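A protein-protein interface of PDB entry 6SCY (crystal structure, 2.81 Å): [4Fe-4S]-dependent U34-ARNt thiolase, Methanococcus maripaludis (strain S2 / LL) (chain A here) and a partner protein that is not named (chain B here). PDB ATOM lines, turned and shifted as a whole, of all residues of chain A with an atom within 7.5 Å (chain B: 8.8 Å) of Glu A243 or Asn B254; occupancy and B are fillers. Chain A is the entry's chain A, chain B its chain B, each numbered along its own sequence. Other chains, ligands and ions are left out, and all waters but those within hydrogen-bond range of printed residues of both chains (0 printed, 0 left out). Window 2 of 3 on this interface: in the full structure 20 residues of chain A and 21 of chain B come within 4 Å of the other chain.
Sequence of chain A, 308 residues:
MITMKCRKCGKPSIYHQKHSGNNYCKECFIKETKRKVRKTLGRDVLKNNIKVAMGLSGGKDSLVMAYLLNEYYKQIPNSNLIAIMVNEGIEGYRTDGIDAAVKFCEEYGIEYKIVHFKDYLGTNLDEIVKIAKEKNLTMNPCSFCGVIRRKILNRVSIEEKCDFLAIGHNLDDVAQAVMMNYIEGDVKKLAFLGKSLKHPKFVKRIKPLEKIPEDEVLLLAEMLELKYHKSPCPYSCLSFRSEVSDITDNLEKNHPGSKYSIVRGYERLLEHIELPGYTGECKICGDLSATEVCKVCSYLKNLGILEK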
ATOM      1  N   GLN A 176      23.864 -31.091  26.245  1.00  0.00           N
ATOM      2  CA  GLN A 176      24.879 -30.353  25.496  1.00  0.00           C
ATOM      3  C   GLN A 176      25.984 -31.266  25.008  1.00  0.00           C
ATOM      4  O   GLN A 176      26.332 -31.210  23.830  1.00  0.00           O
ATOM      5  CB  GLN A 176      25.488 -29.244  26.368  1.00  0.00           C
ATOM      6  CG  GLN A 176      24.563 -28.062  26.586  1.00  0.00           C
ATOM      7  CD  GLN A 176      24.912 -27.279  27.819  1.00  0.00           C
ATOM      8  OE1 GLN A 176      26.033 -27.344  28.340  1.00  0.00           O
ATOM      9  NE2 GLN A 176      23.945 -26.517  28.312  1.00  0.00           N
ATOM     10  N   ILE A 183      27.098 -33.476  16.721  1.00  0.00           N
ATOM     11  CA  ILE A 183      27.579 -32.470  15.752  1.00  0.00           C
ATOM     12  C   ILE A 183      29.021 -32.782  15.284  1.00  0.00           C
ATOM     13  O   ILE A 183      29.328 -32.610  14.101  1.00  0.00           O
ATOM     14  CB  ILE A 183      27.409 -31.001  16.271  1.00  0.00           C
ATOM     15  CG1 ILE A 183      25.933 -30.677  16.578  1.00  0.00           C
ATOM     16  CG2 ILE A 183      27.974 -29.976  15.273  1.00  0.00           C
ATOM     17  CD1 ILE A 183      25.707 -29.612  17.610  1.00  0.00           C
ATOM     18  N   LEU A 238      35.739 -22.360  25.777  1.00  0.00           N
ATOM     19  CA  LEU A 238      35.376 -23.038  24.530  1.00  0.00           C
ATOM     20  C   LEU A 238      34.008 -22.543  24.118  1.00  0.00           C
ATOM     21  O   LEU A 238      33.035 -22.749  24.842  1.00  0.00           O
ATOM     22  CB  LEU A 238      35.364 -24.557  24.701  1.00  0.00           C
ATOM     23  CG  LEU A 238      35.650 -25.318  23.401  1.00  0.00           C
ATOM     24  CD1 LEU A 238      36.768 -26.319  23.682  1.00  0.00           C
ATOM     25  CD2 LEU A 238      34.378 -26.038  22.878  1.00  0.00           C
ATOM     26  N   SER A 239      33.951 -21.812  23.001  1.00  0.00           N
ATOM     27  CA  SER A 239      32.736 -21.170  22.489  1.00  0.00           C
ATOM     28  C   SER A 239      31.719 -22.130  21.865  1.00  0.00           C
ATOM     29  O   SER A 239      30.559 -21.745  21.695  1.00  0.00           O
ATOM     30  CB  SER A 239      33.096 -20.051  21.515  1.00  0.00           C
ATOM     31  OG  SER A 239      33.902 -19.063  22.142  1.00  0.00           O
ATOM     32  N   PHE A 240      32.140 -23.369  21.525  1.00  0.00           N
ATOM     33  CA  PHE A 240      31.257 -24.379  20.929  1.00  0.00           C
ATOM     34  C   PHE A 240      30.159 -24.844  21.889  1.00  0.00           C
ATOM     35  O   PHE A 240      28.999 -24.934  21.478  1.00  0.00           O
ATOM     36  CB  PHE A 240      32.054 -25.562  20.349  1.00  0.00           C
ATOM     37  CG  PHE A 240      31.260 -26.620  19.613  1.00  0.00           C
ATOM     38  CD1 PHE A 240      30.318 -26.265  18.652  1.00  0.00           C
ATOM     39  CD2 PHE A 240      31.499 -27.968  19.833  1.00  0.00           C
ATOM     40  CE1 PHE A 240      29.598 -27.240  17.961  1.00  0.00           C
ATOM     41  CE2 PHE A 240      30.781 -28.945  19.134  1.00  0.00           C
ATOM     42  CZ  PHE A 240      29.834 -28.572  18.205  1.00  0.00           C
ATOM     43  N   ARG A 241      30.518 -25.098  23.171  1.00  0.00           N
ATOM     44  CA  ARG A 241      29.573 -25.511  24.214  1.00  0.00           C
ATOM     45  C   ARG A 241      28.549 -24.401  24.478  1.00  0.00           C
ATOM     46  O   ARG A 241      27.369 -24.701  24.634  1.00  0.00           O
ATOM     47  CB  ARG A 241      30.294 -25.940  25.509  1.00  0.00           C
ATOM     48  CG  ARG A 241      29.423 -26.816  26.414  1.00  0.00           C
ATOM     49  CD  ARG A 241      30.164 -27.332  27.634  1.00  0.00           C
ATOM     50  NE  ARG A 241      29.366 -28.313  28.376  1.00  0.00           N
ATOM     51  CZ  ARG A 241      29.646 -29.613  28.457  1.00  0.00           C
ATOM     52  NH1 ARG A 241      28.862 -30.426  29.147  1.00  0.00           N
ATOM     53  NH2 ARG A 241      30.727 -30.104  27.862  1.00  0.00           N
ATOM     54  N   SER A 242      28.987 -23.123  24.467  1.00  0.00           N
ATOM     55  CA  SER A 242      28.097 -21.972  24.640  1.00  0.00           C
ATOM     56  C   SER A 242      27.175 -21.790  23.416  1.00  0.00           C
ATOM     57  O   SER A 242      26.086 -21.230  23.554  1.00  0.00           O
ATOM     58  CB  SER A 242      28.890 -20.700  24.931  1.00  0.00           C
ATOM     59  OG  SER A 242      29.738 -20.335  23.857  1.00  0.00           O
ATOM     60  N   GLU A 243      27.598 -22.293  22.229  1.00  0.00           N
ATOM     61  CA  GLU A 243      26.806 -22.254  20.995  1.00  0.00           C
ATOM     62  C   GLU A 243      25.781 -23.390  21.042  1.00  0.00           C
ATOM     63  O   GLU A 243      24.610 -23.159  20.736  1.00  0.00           O
ATOM     64  CB  GLU A 243      27.710 -22.385  19.755  1.00  0.00           C
ATOM     65  CG  GLU A 243      27.036 -21.963  18.455  1.00  0.00           C
ATOM     66  CD  GLU A 243      27.721 -22.376  17.165  1.00  0.00           C
ATOM     67  OE1 GLU A 243      28.934 -22.102  17.008  1.00  0.00           O
ATOM     68  OE2 GLU A 243      27.032 -22.959  16.296  1.00  0.00           O
ATOM     69  N   VAL A 244      26.234 -24.608  21.446  1.00  0.00           N
ATOM     70  CA  VAL A 244      25.421 -25.825  21.590  1.00  0.00           C
ATOM     71  C   VAL A 244      24.348 -25.637  22.662  1.00  0.00           C
ATOM     72  O   VAL A 244      23.213 -26.062  22.453  1.00  0.00           O
ATOM     73  CB  VAL A 244      26.291 -27.089  21.820  1.00  0.00           C
ATOM     74  CG1 VAL A 244      25.471 -28.267  22.339  1.00  0.00           C
ATOM     75  CG2 VAL A 244      27.024 -27.480  20.546  1.00  0.00           C
ATOM     76  N   SER A 245      24.700 -24.969  23.789  1.00  0.00           N
ATOM     77  CA  SER A 245      23.769 -24.684  24.888  1.00  0.00           C
ATOM     78  C   SER A 245      22.606 -23.838  24.390  1.00  0.00           C
ATOM     79  O   SER A 245      21.461 -24.113  24.746  1.00  0.00           O
ATOM     80  CB  SER A 245      24.476 -23.998  26.053  1.00  0.00           C
ATOM     81  OG  SER A 245      24.929 -22.701  25.703  1.00  0.00           O
ATOM     82  N   ASP A 246      22.902 -22.861  23.508  1.00  0.00           N
ATOM     83  CA  ASP A 246      21.919 -21.985  22.890  1.00  0.00           C
ATOM     84  C   ASP A 246      20.998 -22.777  21.966  1.00  0.00           C
ATOM     85  O   ASP A 246      19.801 -22.480  21.906  1.00  0.00           O
ATOM     86  CB  ASP A 246      22.614 -20.834  22.144  1.00  0.00           C
ATOM     87  CG  ASP A 246      22.902 -19.608  23.002  1.00  0.00           C
ATOM     88  OD1 ASP A 246      22.506 -18.488  22.592  1.00  0.00           O
ATOM     89  OD2 ASP A 246      23.530 -19.765  24.078  1.00  0.00           O
ATOM     90  N   ILE A 247      21.542 -23.811  21.289  1.00  0.00           N
ATOM     91  CA  ILE A 247      20.782 -24.696  20.401  1.00  0.00           C
ATOM     92  C   ILE A 247      19.769 -25.498  21.243  1.00  0.00           C
ATOM     93  O   ILE A 247      18.572 -25.471  20.943  1.00  0.00           O
ATOM     94  CB  ILE A 247      21.725 -25.605  19.548  1.00  0.00           C
ATOM     95  CG1 ILE A 247      22.548 -24.777  18.540  1.00  0.00           C
ATOM     96  CG2 ILE A 247      20.956 -26.734  18.843  1.00  0.00           C
ATOM     97  CD1 ILE A 247      23.865 -25.397  18.099  1.00  0.00           C
ATOM     98  N   THR A 248      20.264 -26.161  22.320  1.00  0.00           N
ATOM     99  CA  THR A 248      19.484 -26.982  23.258  1.00  0.00           C
ATOM    100  C   THR A 248      18.442 -26.149  24.008  1.00  0.00           C
ATOM    101  O   THR A 248      17.344 -26.645  24.273  1.00  0.00           O
ATOM    102  CB  THR A 248      20.400 -27.773  24.213  1.00  0.00           C
ATOM    103  OG1 THR A 248      21.141 -26.873  25.039  1.00  0.00           O
ATOM    104  CG2 THR A 248      21.338 -28.732  23.482  1.00  0.00           C
ATOM    105  N   ASP A 249      18.786 -24.884  24.333  1.00  0.00           N
ATOM    106  CA  ASP A 249      17.891 -23.954  25.015  1.00  0.00           C
ATOM    107  C   ASP A 249      16.755 -23.528  24.085  1.00  0.00           C
ATOM    108  O   ASP A 249      15.589 -23.641  24.475  1.00  0.00           O
ATOM    109  CB  ASP A 249      18.652 -22.724  25.560  1.00  0.00           C
ATOM    110  CG  ASP A 249      19.464 -22.960  26.825  1.00  0.00           C
ATOM    111  OD1 ASP A 249      19.016 -23.764  27.685  1.00  0.00           O
ATOM    112  OD2 ASP A 249      20.537 -22.326  26.969  1.00  0.00           O
ATOM    113  N   LYS B  18      32.666 -22.271   0.498  1.00  0.00           N
ATOM    114  CA  LYS B  18      32.952 -21.851   1.876  1.00  0.00           C
ATOM    115  C   LYS B  18      33.495 -22.968   2.796  1.00  0.00           C
ATOM    116  O   LYS B  18      34.270 -22.680   3.716  1.00  0.00           O
ATOM    117  CB  LYS B  18      31.721 -21.176   2.499  1.00  0.00           C
ATOM    118  CG  LYS B  18      31.844 -19.656   2.535  1.00  0.00           C
ATOM    119  CD  LYS B  18      30.617 -18.982   3.142  1.00  0.00           C
ATOM    120  CE  LYS B  18      30.875 -17.550   3.562  1.00  0.00           C
ATOM    121  NZ  LYS B  18      31.050 -16.632   2.401  1.00  0.00           N
ATOM    122  N   ASP B 246      17.607 -24.320  10.145  1.00  0.00           N
ATOM    123  CA  ASP B 246      18.208 -23.098  10.675  1.00  0.00           C
ATOM    124  C   ASP B 246      19.338 -23.432  11.643  1.00  0.00           C
ATOM    125  O   ASP B 246      20.344 -22.723  11.661  1.00  0.00           O
ATOM    126  CB  ASP B 246      17.138 -22.208  11.335  1.00  0.00           C
ATOM    127  CG  ASP B 246      16.441 -21.240  10.381  1.00  0.00           C
ATOM    128  OD1 ASP B 246      16.412 -20.025  10.684  1.00  0.00           O
ATOM    129  OD2 ASP B 246      15.924 -21.699   9.328  1.00  0.00           O
ATOM    130  N   ILE B 247      19.192 -24.535  12.405  1.00  0.00           N
ATOM    131  CA  ILE B 247      20.208 -25.020  13.345  1.00  0.00           C
ATOM    132  C   ILE B 247      21.452 -25.471  12.558  1.00  0.00           C
ATOM    133  O   ILE B 247      22.552 -24.983  12.832  1.00  0.00           O
ATOM    134  CB  ILE B 247      19.634 -26.128  14.288  1.00  0.00           C
ATOM    135  CG1 ILE B 247      18.550 -25.556  15.248  1.00  0.00           C
ATOM    136  CG2 ILE B 247      20.751 -26.853  15.061  1.00  0.00           C
ATOM    137  CD1 ILE B 247      17.525 -26.557  15.759  1.00  0.00           C
ATOM    138  N   THR B 248      21.264 -26.368  11.565  1.00  0.00           N
ATOM    139  CA  THR B 248      22.335 -26.895  10.702  1.00  0.00           C
ATOM    140  C   THR B 248      22.991 -25.779   9.894  1.00  0.00           C
ATOM    141  O   THR B 248      24.213 -25.799   9.724  1.00  0.00           O
ATOM    142  CB  THR B 248      21.828 -28.017   9.771  1.00  0.00           C
ATOM    143  OG1 THR B 248      20.830 -27.503   8.891  1.00  0.00           O
ATOM    144  CG2 THR B 248      21.298 -29.234  10.521  1.00  0.00           C
ATOM    145  N   ASP B 249      22.176 -24.807   9.398  1.00  0.00           N
ATOM    146  CA  ASP B 249      22.673 -23.664   8.628  1.00  0.00           C
ATOM    147  C   ASP B 249      23.572 -22.791   9.495  1.00  0.00           C
ATOM    148  O   ASP B 249      24.697 -22.517   9.079  1.00  0.00           O
ATOM    149  CB  ASP B 249      21.534 -22.827   8.008  1.00  0.00           C
ATOM    150  CG  ASP B 249      20.869 -23.433   6.778  1.00  0.00           C
ATOM    151  OD1 ASP B 249      21.572 -24.105   5.986  1.00  0.00           O
ATOM    152  OD2 ASP B 249      19.645 -23.228   6.603  1.00  0.00           O
ATOM    153  N   ASN B 250      23.107 -22.406  10.715  1.00  0.00           N
ATOM    154  CA  ASN B 250      23.888 -21.582  11.646  1.00  0.00           C
ATOM    155  C   ASN B 250      25.119 -22.309  12.176  1.00  0.00           C
ATOM    156  O   ASN B 250      26.098 -21.656  12.540  1.00  0.00           O
ATOM    157  CB  ASN B 250      23.030 -21.013  12.771  1.00  0.00           C
ATOM    158  CG  ASN B 250      22.505 -19.633  12.457  1.00  0.00           C
ATOM    159  OD1 ASN B 250      21.449 -19.466  11.828  1.00  0.00           O
ATOM    160  ND2 ASN B 250      23.236 -18.618  12.887  1.00  0.00           N
ATOM    161  N   LEU B 251      25.084 -23.659  12.178  1.00  0.00           N
ATOM    162  CA  LEU B 251      26.225 -24.485  12.574  1.00  0.00           C
ATOM    163  C   LEU B 251      27.266 -24.464  11.458  1.00  0.00           C
ATOM    164  O   LEU B 251      28.454 -24.361  11.742  1.00  0.00           O
ATOM    165  CB  LEU B 251      25.796 -25.929  12.876  1.00  0.00           C
ATOM    166  CG  LEU B 251      25.412 -26.239  14.310  1.00  0.00           C
ATOM    167  CD1 LEU B 251      24.668 -27.535  14.381  1.00  0.00           C
ATOM    168  CD2 LEU B 251      26.636 -26.306  15.207  1.00  0.00           C
ATOM    169  N   GLU B 252      26.810 -24.548  10.188  1.00  0.00           N
ATOM    170  CA  GLU B 252      27.665 -24.499   9.003  1.00  0.00           C
ATOM    171  C   GLU B 252      28.276 -23.093   8.864  1.00  0.00           C
ATOM    172  O   GLU B 252      29.481 -22.972   8.634  1.00  0.00           O
ATOM    173  CB  GLU B 252      26.855 -24.890   7.755  1.00  0.00           C
ATOM    174  CG  GLU B 252      27.666 -25.023   6.474  1.00  0.00           C
ATOM    175  CD  GLU B 252      28.564 -26.238   6.323  1.00  0.00           C
ATOM    176  OE1 GLU B 252      28.465 -27.177   7.146  1.00  0.00           O
ATOM    177  OE2 GLU B 252      29.369 -26.252   5.365  1.00  0.00           O
ATOM    178  N   LYS B 253      27.448 -22.041   9.067  1.00  0.00           N
ATOM    179  CA  LYS B 253      27.803 -20.618   9.013  1.00  0.00           C
ATOM    180  C   LYS B 253      28.871 -20.230  10.052  1.00  0.00           C
ATOM    181  O   LYS B 253      29.517 -19.196   9.873  1.00  0.00           O
ATOM    182  CB  LYS B 253      26.538 -19.770   9.202  1.00  0.00           C
ATOM    183  CG  LYS B 253      26.586 -18.325   8.723  1.00  0.00           C
ATOM    184  CD  LYS B 253      25.310 -17.580   9.140  1.00  0.00           C
ATOM    185  CE  LYS B 253      25.401 -16.902  10.503  1.00  0.00           C
ATOM    186  NZ  LYS B 253      24.119 -16.273  10.911  1.00  0.00           N
ATOM    187  N   ASN B 254      29.065 -21.049  11.121  1.00  0.00           N
ATOM    188  CA  ASN B 254      30.076 -20.804  12.156  1.00  0.00           C
ATOM    189  C   ASN B 254      31.207 -21.828  12.107  1.00  0.00           C
ATOM    190  O   ASN B 254      32.335 -21.517  12.488  1.00  0.00           O
ATOM    191  CB  ASN B 254      29.446 -20.766  13.549  1.00  0.00           C
ATOM    192  CG  ASN B 254      28.814 -19.445  13.904  1.00  0.00           C
ATOM    193  OD1 ASN B 254      29.403 -18.368  13.721  1.00  0.00           O
ATOM    194  ND2 ASN B 254      27.601 -19.501  14.441  1.00  0.00           N
ATOM    195  N   HIS B 255      30.891 -23.054  11.664  1.00  0.00           N
ATOM    196  CA  HIS B 255      31.828 -24.169  11.567  1.00  0.00           C
ATOM    197  C   HIS B 255      31.619 -24.846  10.213  1.00  0.00           C
ATOM    198  O   HIS B 255      30.727 -25.692  10.095  1.00  0.00           O
ATOM    199  CB  HIS B 255      31.611 -25.174  12.718  1.00  0.00           C
ATOM    200  CG  HIS B 255      31.659 -24.571  14.083  1.00  0.00           C
ATOM    201  ND1 HIS B 255      32.793 -24.656  14.868  1.00  0.00           N
ATOM    202  CD2 HIS B 255      30.704 -23.896  14.762  1.00  0.00           C
ATOM    203  CE1 HIS B 255      32.491 -24.035  15.993  1.00  0.00           C
ATOM    204  NE2 HIS B 255      31.247 -23.555  15.970  1.00  0.00           N
ATOM    205  N   PRO B 256      32.392 -24.459   9.163  1.00  0.00           N
ATOM    206  CA  PRO B 256      32.194 -25.073   7.832  1.00  0.00           C
ATOM    207  C   PRO B 256      32.501 -26.573   7.803  1.00  0.00           C
ATOM    208  O   PRO B 256      33.579 -27.007   8.228  1.00  0.00           O
ATOM    209  CB  PRO B 256      33.114 -24.256   6.906  1.00  0.00           C
ATOM    210  CG  PRO B 256      33.433 -23.013   7.671  1.00  0.00           C
ATOM    211  CD  PRO B 256      33.453 -23.436   9.113  1.00  0.00           C
ATOM    212  N   GLY B 257      31.526 -27.342   7.329  1.00  0.00           N
ATOM    213  CA  GLY B 257      31.607 -28.794   7.236  1.00  0.00           C
ATOM    214  C   GLY B 257      30.848 -29.528   8.325  1.00  0.00           C
ATOM    215  O   GLY B 257      31.046 -30.734   8.505  1.00  0.00           O
ATOM    216  N   SER B 258      29.969 -28.806   9.055  1.00  0.00           N
ATOM    217  CA  SER B 258      29.152 -29.340  10.142  1.00  0.00           C
ATOM    218  C   SER B 258      28.156 -30.363   9.627  1.00  0.00           C
ATOM    219  O   SER B 258      28.120 -31.479  10.139  1.00  0.00           O
ATOM    220  CB  SER B 258      28.447 -28.216  10.891  1.00  0.00           C
ATOM    221  OG  SER B 258      29.373 -27.484  11.675  1.00  0.00           O
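Of the printed residues of chain B, Ile A183 touches Leu B251. No residue of chain B comes within 4 Å of Ser A242. Printed residues of chain B within 4 Å of Glu A243: Leu B251, Asn B254 and His B255. Of the printed residues of chain B, Ile A247 touches Ile B247 (3.8 Å). Printed residues of chain A within 4 Å of Ile B247: Ile A247 (3.8 Å). Of chain A, only Glu A243 (3.7 Å) comes within 4 Å of Asn B254. Of the printed residues of chain A, His B255 touches Phe A240 (3.9 Å) and Glu A243 (2.9 Å). The nearest residue of chain B that does not touch Glu A243 is Asn B250 (4.1 Å).
Hydrophobic or aromatic side chains of chain A that line the printed part of chain B: Ile A183, Phe A240 and Ile A247. Of the 14 printed residues of chain B, 4 touch a printed residue of chain A. Printed residues of chain B that touch a printed residue of chain A: Ile B247, Leu B251, Asn B254 and His B255. Among the printed residues, 6 pairs touch across the chains.
The side-chain carboxylate of Glu A243 sits at hydrogen-bond distance from a ring nitrogen (NE2) of His B255.
O of Asn B250 sits at hydrogen-bond distance from ND2 of Asn B254 (3.2 Å). O of Leu B251 lies within hydrogen-bond range of OG of Ser B258 (3.3 Å). OG of Ser B258 sits at hydrogen-bond distance from O of His B255.
Leu B251 touches Ile A183. CD1 of Phe A240 touches NE2 of His B255 (3.9 Å). Glu A243 touches Leu B251 (OE2 to CD2, 3.5 Å). OE1 of Glu A243 touches CB of Asn B254, 3.7 Å away. Ile A247 touches Ile B247.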
